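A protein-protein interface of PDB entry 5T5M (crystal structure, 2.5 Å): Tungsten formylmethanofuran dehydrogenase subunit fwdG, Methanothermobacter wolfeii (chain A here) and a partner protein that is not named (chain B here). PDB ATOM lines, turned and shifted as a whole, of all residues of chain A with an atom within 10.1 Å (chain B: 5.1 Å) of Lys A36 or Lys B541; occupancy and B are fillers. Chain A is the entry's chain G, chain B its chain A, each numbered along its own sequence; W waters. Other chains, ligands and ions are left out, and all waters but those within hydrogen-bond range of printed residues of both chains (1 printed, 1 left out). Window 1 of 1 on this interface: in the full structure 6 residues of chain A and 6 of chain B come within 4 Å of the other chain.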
ATOM      1  N   CYS A  15     -24.657  37.163 -31.591  1.00  0.00           N
ATOM      2  CA  CYS A  15     -23.729  36.045 -31.589  1.00  0.00           C
ATOM      3  C   CYS A  15     -23.586  35.406 -30.210  1.00  0.00           C
ATOM      4  O   CYS A  15     -23.188  34.242 -30.118  1.00  0.00           O
ATOM      5  CB  CYS A  15     -22.372  36.532 -32.103  1.00  0.00           C
ATOM      6  SG  CYS A  15     -21.298  37.251 -30.831  1.00  0.00           S
ATOM      7  N   GLY A  16     -23.877  36.145 -29.143  1.00  0.00           N
ATOM      8  CA  GLY A  16     -23.889  35.582 -27.815  1.00  0.00           C
ATOM      9  C   GLY A  16     -22.579  35.654 -27.067  1.00  0.00           C
ATOM     10  O   GLY A  16     -22.544  35.265 -25.892  1.00  0.00           O
ATOM     11  N   ASN A  17     -21.498  36.126 -27.700  1.00  0.00           N
ATOM     12  CA  ASN A  17     -20.219  36.215 -26.998  1.00  0.00           C
ATOM     13  C   ASN A  17     -20.399  36.887 -25.644  1.00  0.00           C
ATOM     14  O   ASN A  17     -19.971  36.363 -24.609  1.00  0.00           O
ATOM     15  CB  ASN A  17     -19.197  36.987 -27.837  1.00  0.00           C
ATOM     16  CG  ASN A  17     -18.744  36.219 -29.061  1.00  0.00           C
ATOM     17  OD1 ASN A  17     -19.250  35.137 -29.346  1.00  0.00           O
ATOM     18  ND2 ASN A  17     -17.789  36.782 -29.799  1.00  0.00           N
ATOM     19  N   CYS A  18     -21.052  38.048 -25.640  1.00  0.00           N
ATOM     20  CA  CYS A  18     -21.173  38.844 -24.425  1.00  0.00           C
ATOM     21  C   CYS A  18     -21.918  38.077 -23.338  1.00  0.00           C
ATOM     22  O   CYS A  18     -21.487  38.046 -22.180  1.00  0.00           O
ATOM     23  CB  CYS A  18     -21.884  40.156 -24.751  1.00  0.00           C
ATOM     24  SG  CYS A  18     -23.625  39.973 -25.125  1.00  0.00           S
ATOM     25  N   VAL A  19     -23.030  37.436 -23.695  1.00  0.00           N
ATOM     26  CA  VAL A  19     -23.819  36.709 -22.709  1.00  0.00           C
ATOM     27  C   VAL A  19     -22.970  35.641 -22.031  1.00  0.00           C
ATOM     28  O   VAL A  19     -23.059  35.439 -20.811  1.00  0.00           O
ATOM     29  CB  VAL A  19     -25.068  36.097 -23.365  1.00  0.00           C
ATOM     30  CG1 VAL A  19     -25.833  35.262 -22.353  1.00  0.00           C
ATOM     31  CG2 VAL A  19     -25.963  37.189 -23.943  1.00  0.00           C
ATOM     32  N   ILE A  20     -22.150  34.928 -22.809  1.00  0.00           N
ATOM     33  CA  ILE A  20     -21.359  33.832 -22.260  1.00  0.00           C
ATOM     34  C   ILE A  20     -20.195  34.367 -21.436  1.00  0.00           C
ATOM     35  O   ILE A  20     -19.888  33.844 -20.354  1.00  0.00           O
ATOM     36  CB  ILE A  20     -20.866  32.921 -23.399  1.00  0.00           C
ATOM     37  CG1 ILE A  20     -22.041  32.422 -24.253  1.00  0.00           C
ATOM     38  CG2 ILE A  20     -20.060  31.769 -22.840  1.00  0.00           C
ATOM     39  CD1 ILE A  20     -23.233  31.904 -23.454  1.00  0.00           C
ATOM     40  N   ALA A  21     -19.518  35.401 -21.939  1.00  0.00           N
ATOM     41  CA  ALA A  21     -18.333  35.923 -21.264  1.00  0.00           C
ATOM     42  C   ALA A  21     -18.674  36.542 -19.914  1.00  0.00           C
ATOM     43  O   ALA A  21     -17.831  36.570 -19.010  1.00  0.00           O
ATOM     44  CB  ALA A  21     -17.641  36.956 -22.159  1.00  0.00           C
ATOM     45  N   CYS A  22     -19.892  37.034 -19.756  1.00  0.00           N
ATOM     46  CA  CYS A  22     -20.248  37.769 -18.557  1.00  0.00           C
ATOM     47  C   CYS A  22     -20.102  36.889 -17.317  1.00  0.00           C
ATOM     48  O   CYS A  22     -20.773  35.853 -17.226  1.00  0.00           O
ATOM     49  CB  CYS A  22     -21.676  38.282 -18.667  1.00  0.00           C
ATOM     50  SG  CYS A  22     -22.329  38.856 -17.082  1.00  0.00           S
ATOM     51  N   ASN A  25     -23.573  36.526 -15.513  1.00  0.00           N
ATOM     52  CA  ASN A  25     -24.432  35.556 -16.180  1.00  0.00           C
ATOM     53  C   ASN A  25     -23.952  34.144 -15.902  1.00  0.00           C
ATOM     54  O   ASN A  25     -24.757  33.256 -15.597  1.00  0.00           O
ATOM     55  CB  ASN A  25     -24.462  35.802 -17.684  1.00  0.00           C
ATOM     56  CG  ASN A  25     -25.028  37.147 -18.052  1.00  0.00           C
ATOM     57  OD1 ASN A  25     -25.629  37.830 -17.226  1.00  0.00           O
ATOM     58  ND2 ASN A  25     -24.842  37.542 -19.314  1.00  0.00           N
ATOM     59  N   ALA A  26     -22.636  33.924 -15.997  1.00  0.00           N
ATOM     60  CA  ALA A  26     -22.082  32.587 -15.815  1.00  0.00           C
ATOM     61  C   ALA A  26     -22.351  32.074 -14.411  1.00  0.00           C
ATOM     62  O   ALA A  26     -22.737  30.915 -14.227  1.00  0.00           O
ATOM     63  CB  ALA A  26     -20.579  32.598 -16.102  1.00  0.00           C
ATOM     64  N   ARG A  28     -24.753  32.713 -12.466  1.00  0.00           N
ATOM     65  CA  ARG A  28     -26.168  32.460 -12.235  1.00  0.00           C
ATOM     66  C   ARG A  28     -26.742  31.339 -13.087  1.00  0.00           C
ATOM     67  O   ARG A  28     -27.742  30.731 -12.689  1.00  0.00           O
ATOM     68  CB  ARG A  28     -26.963  33.736 -12.496  1.00  0.00           C
ATOM     69  CG  ARG A  28     -26.716  34.810 -11.459  1.00  0.00           C
ATOM     70  CD  ARG A  28     -27.187  36.149 -11.955  1.00  0.00           C
ATOM     71  NE  ARG A  28     -27.234  37.154 -10.899  1.00  0.00           N
ATOM     72  CZ  ARG A  28     -28.316  37.441 -10.185  1.00  0.00           C
ATOM     73  NH1 ARG A  28     -29.458  36.804 -10.399  1.00  0.00           N
ATOM     74  NH2 ARG A  28     -28.258  38.378  -9.253  1.00  0.00           N
ATOM     75  N   SER A  29     -26.145  31.050 -14.239  1.00  0.00           N
ATOM     76  CA  SER A  29     -26.649  30.014 -15.142  1.00  0.00           C
ATOM     77  C   SER A  29     -25.531  29.072 -15.582  1.00  0.00           C
ATOM     78  O   SER A  29     -24.648  29.482 -16.366  1.00  0.00           O
ATOM     79  CB  SER A  29     -27.310  30.643 -16.360  1.00  0.00           C
ATOM     80  OG  SER A  29     -27.775  29.629 -17.234  1.00  0.00           O
ATOM     81  N   PRO A  30     -25.535  27.818 -15.124  1.00  0.00           N
ATOM     82  CA  PRO A  30     -24.584  26.831 -15.661  1.00  0.00           C
ATOM     83  C   PRO A  30     -24.677  26.651 -17.167  1.00  0.00           C
ATOM     84  O   PRO A  30     -23.671  26.312 -17.805  1.00  0.00           O
ATOM     85  CB  PRO A  30     -24.973  25.541 -14.926  1.00  0.00           C
ATOM     86  CG  PRO A  30     -25.650  26.001 -13.669  1.00  0.00           C
ATOM     87  CD  PRO A  30     -26.338  27.279 -14.015  1.00  0.00           C
ATOM     88  N   GLU A  31     -25.857  26.853 -17.755  1.00  0.00           N
ATOM     89  CA  GLU A  31     -25.983  26.759 -19.205  1.00  0.00           C
ATOM     90  C   GLU A  31     -25.190  27.868 -19.886  1.00  0.00           C
ATOM     91  O   GLU A  31     -24.403  27.611 -20.803  1.00  0.00           O
ATOM     92  CB  GLU A  31     -27.458  26.809 -19.607  1.00  0.00           C
ATOM     93  CG  GLU A  31     -28.214  25.550 -19.240  1.00  0.00           C
ATOM     94  CD  GLU A  31     -29.703  25.668 -19.463  1.00  0.00           C
ATOM     95  OE1 GLU A  31     -30.325  26.602 -18.909  1.00  0.00           O
ATOM     96  OE2 GLU A  31     -30.249  24.823 -20.198  1.00  0.00           O
ATOM     97  N   VAL A  32     -25.377  29.112 -19.436  1.00  0.00           N
ATOM     98  CA  VAL A  32     -24.602  30.236 -19.959  1.00  0.00           C
ATOM     99  C   VAL A  32     -23.118  30.001 -19.739  1.00  0.00           C
ATOM    100  O   VAL A  32     -22.298  30.193 -20.643  1.00  0.00           O
ATOM    101  CB  VAL A  32     -25.050  31.548 -19.297  1.00  0.00           C
ATOM    102  CG1 VAL A  32     -24.093  32.675 -19.645  1.00  0.00           C
ATOM    103  CG2 VAL A  32     -26.478  31.894 -19.703  1.00  0.00           C
ATOM    104  N   ALA A  33     -22.748  29.624 -18.515  1.00  0.00           N
ATOM    105  CA  ALA A  33     -21.350  29.357 -18.216  1.00  0.00           C
ATOM    106  C   ALA A  33     -20.729  28.450 -19.268  1.00  0.00           C
ATOM    107  O   ALA A  33     -19.552  28.604 -19.620  1.00  0.00           O
ATOM    108  CB  ALA A  33     -21.236  28.737 -16.822  1.00  0.00           C
ATOM    109  N   GLY A  34     -21.514  27.516 -19.801  1.00  0.00           N
ATOM    110  CA  GLY A  34     -21.029  26.558 -20.781  1.00  0.00           C
ATOM    111  C   GLY A  34     -21.278  26.930 -22.226  1.00  0.00           C
ATOM    112  O   GLY A  34     -21.217  26.073 -23.115  1.00  0.00           O
ATOM    113  N   GLY A  35     -21.563  28.200 -22.484  1.00  0.00           N
ATOM    114  CA  GLY A  35     -21.719  28.683 -23.838  1.00  0.00           C
ATOM    115  C   GLY A  35     -23.104  28.542 -24.419  1.00  0.00           C
ATOM    116  O   GLY A  35     -23.295  28.857 -25.601  1.00  0.00           O
ATOM    117  N   LYS A  36     -24.069  28.071 -23.639  1.00  0.00           N
ATOM    118  CA  LYS A  36     -25.436  27.898 -24.099  1.00  0.00           C
ATOM    119  C   LYS A  36     -26.284  29.090 -23.685  1.00  0.00           C
ATOM    120  O   LYS A  36     -26.033  29.732 -22.664  1.00  0.00           O
ATOM    121  CB  LYS A  36     -26.046  26.625 -23.521  1.00  0.00           C
ATOM    122  CG  LYS A  36     -25.417  25.345 -24.011  1.00  0.00           C
ATOM    123  CD  LYS A  36     -25.897  24.203 -23.169  1.00  0.00           C
ATOM    124  CE  LYS A  36     -25.487  22.869 -23.741  1.00  0.00           C
ATOM    125  NZ  LYS A  36     -26.102  21.771 -22.924  1.00  0.00           N
ATOM    126  N   GLY A  37     -27.297  29.383 -24.488  1.00  0.00           N
ATOM    127  CA  GLY A  37     -28.328  30.292 -24.062  1.00  0.00           C
ATOM    128  C   GLY A  37     -29.112  29.637 -22.947  1.00  0.00           C
ATOM    129  O   GLY A  37     -29.303  28.414 -22.940  1.00  0.00           O
ATOM    130  N   PRO A  38     -29.568  30.422 -21.969  1.00  0.00           N
ATOM    131  CA  PRO A  38     -30.334  29.827 -20.871  1.00  0.00           C
ATOM    132  C   PRO A  38     -31.641  29.264 -21.390  1.00  0.00           C
ATOM    133  O   PRO A  38     -32.315  29.881 -22.217  1.00  0.00           O
ATOM    134  CB  PRO A  38     -30.563  31.001 -19.910  1.00  0.00           C
ATOM    135  CG  PRO A  38     -30.602  32.188 -20.800  1.00  0.00           C
ATOM    136  CD  PRO A  38     -29.573  31.895 -21.892  1.00  0.00           C
ATOM    137  N   THR A  39     -31.971  28.064 -20.930  1.00  0.00           N
ATOM    138  CA  THR A  39     -33.291  27.481 -21.124  1.00  0.00           C
ATOM    139  C   THR A  39     -34.087  27.523 -19.832  1.00  0.00           C
ATOM    140  O   THR A  39     -35.253  27.919 -19.833  1.00  0.00           O
ATOM    141  CB  THR A  39     -33.164  26.042 -21.636  1.00  0.00           C
ATOM    142  OG1 THR A  39     -32.499  26.050 -22.906  1.00  0.00           O
ATOM    143  CG2 THR A  39     -34.514  25.395 -21.792  1.00  0.00           C
ATOM    144  N   ASP A  40     -33.464  27.120 -18.727  1.00  0.00           N
ATOM    145  CA  ASP A  40     -34.009  27.397 -17.411  1.00  0.00           C
ATOM    146  C   ASP A  40     -34.266  28.892 -17.258  1.00  0.00           C
ATOM    147  O   ASP A  40     -33.474  29.721 -17.713  1.00  0.00           O
ATOM    148  CB  ASP A  40     -33.033  26.916 -16.336  1.00  0.00           C
ATOM    149  CG  ASP A  40     -32.879  25.409 -16.313  1.00  0.00           C
ATOM    150  OD1 ASP A  40     -33.787  24.704 -16.806  1.00  0.00           O
ATOM    151  OD2 ASP A  40     -31.854  24.930 -15.783  1.00  0.00           O
ATOM    152  N   ASP A  41     -35.390  29.233 -16.623  1.00  0.00           N
ATOM    153  CA  ASP A  41     -35.678  30.625 -16.293  1.00  0.00           C
ATOM    154  C   ASP A  41     -34.673  31.094 -15.252  1.00  0.00           C
ATOM    155  O   ASP A  41     -34.632  30.568 -14.134  1.00  0.00           O
ATOM    156  CB  ASP A  41     -37.104  30.784 -15.769  1.00  0.00           C
ATOM    157  CG  ASP A  41     -38.115  30.972 -16.878  1.00  0.00           C
ATOM    158  OD1 ASP A  41     -37.685  31.213 -18.025  1.00  0.00           O
ATOM    159  OD2 ASP A  41     -39.332  30.895 -16.597  1.00  0.00           O
ATOM    160  N   VAL A  42     -33.855  32.071 -15.622  1.00  0.00           N
ATOM    161  CA  VAL A  42     -32.868  32.659 -14.732  1.00  0.00           C
ATOM    162  C   VAL A  42     -32.864  34.161 -14.988  1.00  0.00           C
ATOM    163  O   VAL A  42     -33.230  34.628 -16.071  1.00  0.00           O
ATOM    164  CB  VAL A  42     -31.472  32.016 -14.932  1.00  0.00           C
ATOM    165  CG1 VAL A  42     -31.229  31.650 -16.401  1.00  0.00           C
ATOM    166  CG2 VAL A  42     -30.373  32.933 -14.439  1.00  0.00           C
ATOM    167  N   ILE A  44     -30.620  37.138 -15.475  1.00  0.00           N
ATOM    168  CA  ILE A  44     -29.255  37.561 -15.776  1.00  0.00           C
ATOM    169  C   ILE A  44     -29.276  38.975 -16.346  1.00  0.00           C
ATOM    170  O   ILE A  44     -30.342  39.577 -16.508  1.00  0.00           O
ATOM    171  CB  ILE A  44     -28.556  36.584 -16.740  1.00  0.00           C
ATOM    172  CG1 ILE A  44     -29.411  36.315 -17.988  1.00  0.00           C
ATOM    173  CG2 ILE A  44     -28.216  35.293 -16.009  1.00  0.00           C
ATOM    174  CD1 ILE A  44     -28.783  35.331 -18.957  1.00  0.00           C
ATOM    175  N   MET A  46     -28.282  40.223 -19.365  1.00  0.00           N
ATOM    176  CA  MET A  46     -28.781  40.378 -20.719  1.00  0.00           C
ATOM    177  C   MET A  46     -28.813  39.015 -21.382  1.00  0.00           C
ATOM    178  O   MET A  46     -28.188  38.055 -20.921  1.00  0.00           O
ATOM    179  CB  MET A  46     -27.927  41.357 -21.531  1.00  0.00           C
ATOM    180  CG  MET A  46     -26.529  40.864 -21.897  1.00  0.00           C
ATOM    181  SD  MET A  46     -25.391  40.874 -20.491  1.00  0.00           S
ATOM    182  CE  MET A  46     -23.901  41.470 -21.285  1.00  0.00           C
ATOM    183  N   ILE A  47     -29.586  38.948 -22.458  1.00  0.00           N
ATOM    184  CA  ILE A  47     -29.683  37.791 -23.330  1.00  0.00           C
ATOM    185  C   ILE A  47     -29.714  38.302 -24.760  1.00  0.00           C
ATOM    186  O   ILE A  47     -29.760  39.507 -25.014  1.00  0.00           O
ATOM    187  CB  ILE A  47     -30.950  36.954 -23.073  1.00  0.00           C
ATOM    188  CG1 ILE A  47     -32.170  37.883 -23.087  1.00  0.00           C
ATOM    189  CG2 ILE A  47     -30.824  36.154 -21.804  1.00  0.00           C
ATOM    190  CD1 ILE A  47     -33.484  37.179 -22.908  1.00  0.00           C
ATOM    191  N   VAL A  48     -29.716  37.358 -25.693  1.00  0.00           N
ATOM    192  CA  VAL A  48     -30.081  37.626 -27.076  1.00  0.00           C
ATOM    193  C   VAL A  48     -31.566  37.320 -27.206  1.00  0.00           C
ATOM    194  O   VAL A  48     -31.998  36.185 -26.975  1.00  0.00           O
ATOM    195  CB  VAL A  48     -29.244  36.782 -28.049  1.00  0.00           C
ATOM    196  CG1 VAL A  48     -29.693  37.011 -29.478  1.00  0.00           C
ATOM    197  CG2 VAL A  48     -27.756  37.108 -27.894  1.00  0.00           C
ATOM    198  N   GLU B 537     -28.852  15.424 -16.089  1.00  0.00           N
ATOM    199  CA  GLU B 537     -29.312  16.639 -16.749  1.00  0.00           C
ATOM    200  C   GLU B 537     -28.479  17.841 -16.325  1.00  0.00           C
ATOM    201  O   GLU B 537     -28.157  18.702 -17.153  1.00  0.00           O
ATOM    202  CB  GLU B 537     -30.789  16.876 -16.451  1.00  0.00           C
ATOM    203  CG  GLU B 537     -31.297  18.197 -17.001  1.00  0.00           C
ATOM    204  CD  GLU B 537     -32.804  18.245 -17.136  1.00  0.00           C
ATOM    205  OE1 GLU B 537     -33.290  19.093 -17.918  1.00  0.00           O
ATOM    206  OE2 GLU B 537     -33.495  17.444 -16.464  1.00  0.00           O
ATOM    207  N   SER B 538     -28.118  17.917 -15.040  1.00  0.00           N
ATOM    208  CA  SER B 538     -27.263  19.002 -14.571  1.00  0.00           C
ATOM    209  C   SER B 538     -25.914  19.009 -15.286  1.00  0.00           C
ATOM    210  O   SER B 538     -25.346  20.080 -15.533  1.00  0.00           O
ATOM    211  CB  SER B 538     -27.059  18.891 -13.062  1.00  0.00           C
ATOM    212  OG  SER B 538     -25.935  19.651 -12.645  1.00  0.00           O
ATOM    213  N   LYS B 539     -25.380  17.829 -15.613  1.00  0.00           N
ATOM    214  CA  LYS B 539     -24.114  17.762 -16.336  1.00  0.00           C
ATOM    215  C   LYS B 539     -24.282  18.138 -17.797  1.00  0.00           C
ATOM    216  O   LYS B 539     -23.370  18.727 -18.382  1.00  0.00           O
ATOM    217  CB  LYS B 539     -23.508  16.356 -16.226  1.00  0.00           C
ATOM    218  CG  LYS B 539     -23.018  15.988 -14.835  1.00  0.00           C
ATOM    219  CD  LYS B 539     -21.845  16.843 -14.394  1.00  0.00           C
ATOM    220  CE  LYS B 539     -21.886  17.137 -12.896  1.00  0.00           C
ATOM    221  NZ  LYS B 539     -21.681  15.923 -12.058  1.00  0.00           N
ATOM    222  N   PHE B 540     -25.430  17.807 -18.395  1.00  0.00           N
ATOM    223  CA  PHE B 540     -25.705  18.213 -19.767  1.00  0.00           C
ATOM    224  C   PHE B 540     -25.700  19.727 -19.900  1.00  0.00           C
ATOM    225  O   PHE B 540     -25.147  20.274 -20.862  1.00  0.00           O
ATOM    226  CB  PHE B 540     -27.052  17.654 -20.220  1.00  0.00           C
ATOM    227  CG  PHE B 540     -26.964  16.327 -20.918  1.00  0.00           C
ATOM    228  CD1 PHE B 540     -26.833  15.142 -20.200  1.00  0.00           C
ATOM    229  CD2 PHE B 540     -27.052  16.263 -22.291  1.00  0.00           C
ATOM    230  CE1 PHE B 540     -26.768  13.920 -20.858  1.00  0.00           C
ATOM    231  CE2 PHE B 540     -26.982  15.053 -22.954  1.00  0.00           C
ATOM    232  CZ  PHE B 540     -26.840  13.883 -22.243  1.00  0.00           C
ATOM    233  N   LYS B 541     -26.316  20.424 -18.946  1.00  0.00           N
ATOM    234  CA  LYS B 541     -26.338  21.881 -18.994  1.00  0.00           C
ATOM    235  C   LYS B 541     -24.932  22.465 -18.981  1.00  0.00           C
ATOM    236  O   LYS B 541     -24.690  23.504 -19.603  1.00  0.00           O
ATOM    237  CB  LYS B 541     -27.133  22.431 -17.813  1.00  0.00           C
ATOM    238  CG  LYS B 541     -28.553  21.921 -17.737  1.00  0.00           C
ATOM    239  CD  LYS B 541     -29.264  22.449 -16.515  1.00  0.00           C
ATOM    240  CE  LYS B 541     -30.654  21.895 -16.440  1.00  0.00           C
ATOM    241  NZ  LYS B 541     -31.321  22.252 -15.166  1.00  0.00           N
ATOM    242  N   GLN B 542     -23.998  21.816 -18.280  1.00  0.00           N
ATOM    243  CA  GLN B 542     -22.646  22.337 -18.093  1.00  0.00           C
ATOM    244  C   GLN B 542     -21.703  21.953 -19.237  1.00  0.00           C
ATOM    245  O   GLN B 542     -20.991  22.812 -19.769  1.00  0.00           O
ATOM    246  CB  GLN B 542     -22.065  21.826 -16.762  1.00  0.00           C
ATOM    247  CG  GLN B 542     -22.779  22.315 -15.493  1.00  0.00           C
ATOM    248  CD  GLN B 542     -22.085  21.865 -14.204  1.00  0.00           C
ATOM    249  OE1 GLN B 542     -22.462  20.862 -13.601  1.00  0.00           O
ATOM    250  NE2 GLN B 542     -21.073  22.612 -13.780  1.00  0.00           N
ATOM    251  N   TYR B 543     -21.693  20.671 -19.626  1.00  0.00           N
ATOM    252  CA  TYR B 543     -20.595  20.107 -20.394  1.00  0.00           C
ATOM    253  C   TYR B 543     -20.979  19.520 -21.747  1.00  0.00           C
ATOM    254  O   TYR B 543     -20.109  19.423 -22.615  1.00  0.00           O
ATOM    255  CB  TYR B 543     -19.886  19.020 -19.569  1.00  0.00           C
ATOM    256  CG  TYR B 543     -19.409  19.536 -18.239  1.00  0.00           C
ATOM    257  CD1 TYR B 543     -18.547  20.622 -18.166  1.00  0.00           C
ATOM    258  CD2 TYR B 543     -19.832  18.957 -17.054  1.00  0.00           C
ATOM    259  CE1 TYR B 543     -18.113  21.110 -16.951  1.00  0.00           C
ATOM    260  CE2 TYR B 543     -19.405  19.432 -15.831  1.00  0.00           C
ATOM    261  CZ  TYR B 543     -18.547  20.508 -15.779  1.00  0.00           C
ATOM    262  OH  TYR B 543     -18.123  20.978 -14.550  1.00  0.00           O
ATOM    263  N   TYR B 544     -22.224  19.115 -21.955  1.00  0.00           N
ATOM    264  CA  TYR B 544     -22.603  18.631 -23.269  1.00  0.00           C
ATOM    265  C   TYR B 544     -22.808  19.812 -24.206  1.00  0.00           C
ATOM    266  O   TYR B 544     -23.009  20.951 -23.771  1.00  0.00           O
ATOM    267  CB  TYR B 544     -23.877  17.786 -23.194  1.00  0.00           C
ATOM    268  CG  TYR B 544     -23.640  16.284 -23.181  1.00  0.00           C
ATOM    269  CD1 TYR B 544     -23.433  15.585 -24.368  1.00  0.00           C
ATOM    270  CD2 TYR B 544     -23.636  15.567 -21.989  1.00  0.00           C
ATOM    271  CE1 TYR B 544     -23.225  14.213 -24.369  1.00  0.00           C
ATOM    272  CE2 TYR B 544     -23.424  14.191 -21.975  1.00  0.00           C
ATOM    273  CZ  TYR B 544     -23.221  13.523 -23.167  1.00  0.00           C
ATOM    274  OH  TYR B 544     -23.016  12.167 -23.157  1.00  0.00           O
ATOM    275  N   SER B 545     -22.731  19.535 -25.509  1.00  0.00           N
ATOM    276  CA  SER B 545     -22.976  20.536 -26.542  1.00  0.00           C
ATOM    277  C   SER B 545     -24.408  20.508 -27.061  1.00  0.00           C
ATOM    278  O   SER B 545     -24.707  21.179 -28.052  1.00  0.00           O
ATOM    279  CB  SER B 545     -22.014  20.338 -27.700  1.00  0.00           C
ATOM    280  OG  SER B 545     -22.368  19.179 -28.428  1.00  0.00           O
ATOM    281  N   VAL B 546     -25.291  19.747 -26.413  1.00  0.00           N
ATOM    282  CA  VAL B 546     -26.693  19.640 -26.784  1.00  0.00           C
ATOM    283  C   VAL B 546     -27.527  19.752 -25.514  1.00  0.00           C
ATOM    284  O   VAL B 546     -27.059  19.480 -24.408  1.00  0.00           O
ATOM    285  CB  VAL B 546     -27.007  18.317 -27.512  1.00  0.00           C
ATOM    286  CG1 VAL B 546     -26.245  18.224 -28.817  1.00  0.00           C
ATOM    287  CG2 VAL B 546     -26.663  17.128 -26.612  1.00  0.00           C
ATOM    288  N   ASN B 547     -28.780  20.154 -25.684  1.00  0.00           N
ATOM    289  CA  ASN B 547     -29.681  20.258 -24.547  1.00  0.00           C
ATOM    290  C   ASN B 547     -30.242  18.883 -24.197  1.00  0.00           C
ATOM    291  O   ASN B 547     -30.520  18.061 -25.076  1.00  0.00           O
ATOM    292  CB  ASN B 547     -30.803  21.253 -24.835  1.00  0.00           C
ATOM    293  CG  ASN B 547     -30.432  22.677 -24.433  1.00  0.00           C
ATOM    294  OD1 ASN B 547     -29.277  22.968 -24.130  1.00  0.00           O
ATOM    295  ND2 ASN B 547     -31.410  23.563 -24.421  1.00  0.00           N
HETATM  296  O   HOH W   1     -21.085  24.941 -16.252  1.00  0.00           O
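O of Phe B540 sits at hydrogen-bond distance from NZ of Lys A36 (2.7 Å).
NZ of Lys B541 lies within salt-bridge range of OD2 of Asp A40 (2.8 Å).
The backbone carbonyl oxygen of Tyr B544 sits close to the side-chain amino group of Lys A36, at 3.3 Å.
O of Val B546 sits at hydrogen-bond distance from NZ of Lys A36 (2.9 Å).
The side-chain amide nitrogen (ND2) of Asn B547 sits at hydrogen-bond distance from the side-chain hydroxyl (OG1) of Thr A39 (3.1 Å).
O of Lys B541 sits close to O of Pro A30, at 3.5 Å.
NE2 of Gln B542 sits at hydrogen-bond distance from OH of Tyr B543, 3.5 Å away.
The side-chain hydroxyl (OG) of Ser A29 lies close to the backbone NH (N) of Glu A31, 3.4 Å away.
O of Glu A31 lies within hydrogen-bond range of N of Lys A36.
The backbone NH (N) of Thr A39 is in hydrogen-bond range of the side-chain carboxylate (OE1) of Glu A31 (3.0 Å).
OE1 of Glu A31 is in hydrogen-bond range of N of Asp A40.
Among the printed residues, merely in contact across the chains: Glu A31 with Lys B541 (3.5 Å), Lys A36 with Asn B547 (3.6 Å), Lys A36 with Lys B541 (3.8 Å), Gly A34 with Gln B542 (3.9 Å) and Pro A30 with Gln B542 (3.9 Å).
Of the printed residues of chain B, Lys A36 touches Phe B540, Lys B541, Tyr B544, Val B546 and Asn B547.
Lys B541 touches four residues of chain A.
Printed residues of chain A within 4 Å of Gln B542: Pro A30 (3.9 Å) and Gly A34 (3.9 Å).
Of the printed residues of chain B, Asp A40 touches Lys B541.
Gly A37 touches none of the printed residues of chain B.
Glu B537 touches none of the printed residues of chain A.
The nearest residue of chain B that does not touch Lys A36 is Ser B545 (4.2 Å).
The nearest residue of chain A that does not touch Lys B541 is Gly A34 (4.9 Å).
Of the 29 printed residues of chain A, 6 touch a printed residue of chain B.
Printed residues of chain B that touch a printed residue of chain A: Phe B540, Lys B541, Gln B542, Tyr B544, Val B546 and Asn B547.
Among the printed residues, 11 pairs touch across the chains.
Water W1 lies within hydrogen-bond range of the backbone carbonyl oxygen of Pro A30 (3.3 Å) and the side-chain amide nitrogen of Gln B542 (3.4 Å).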
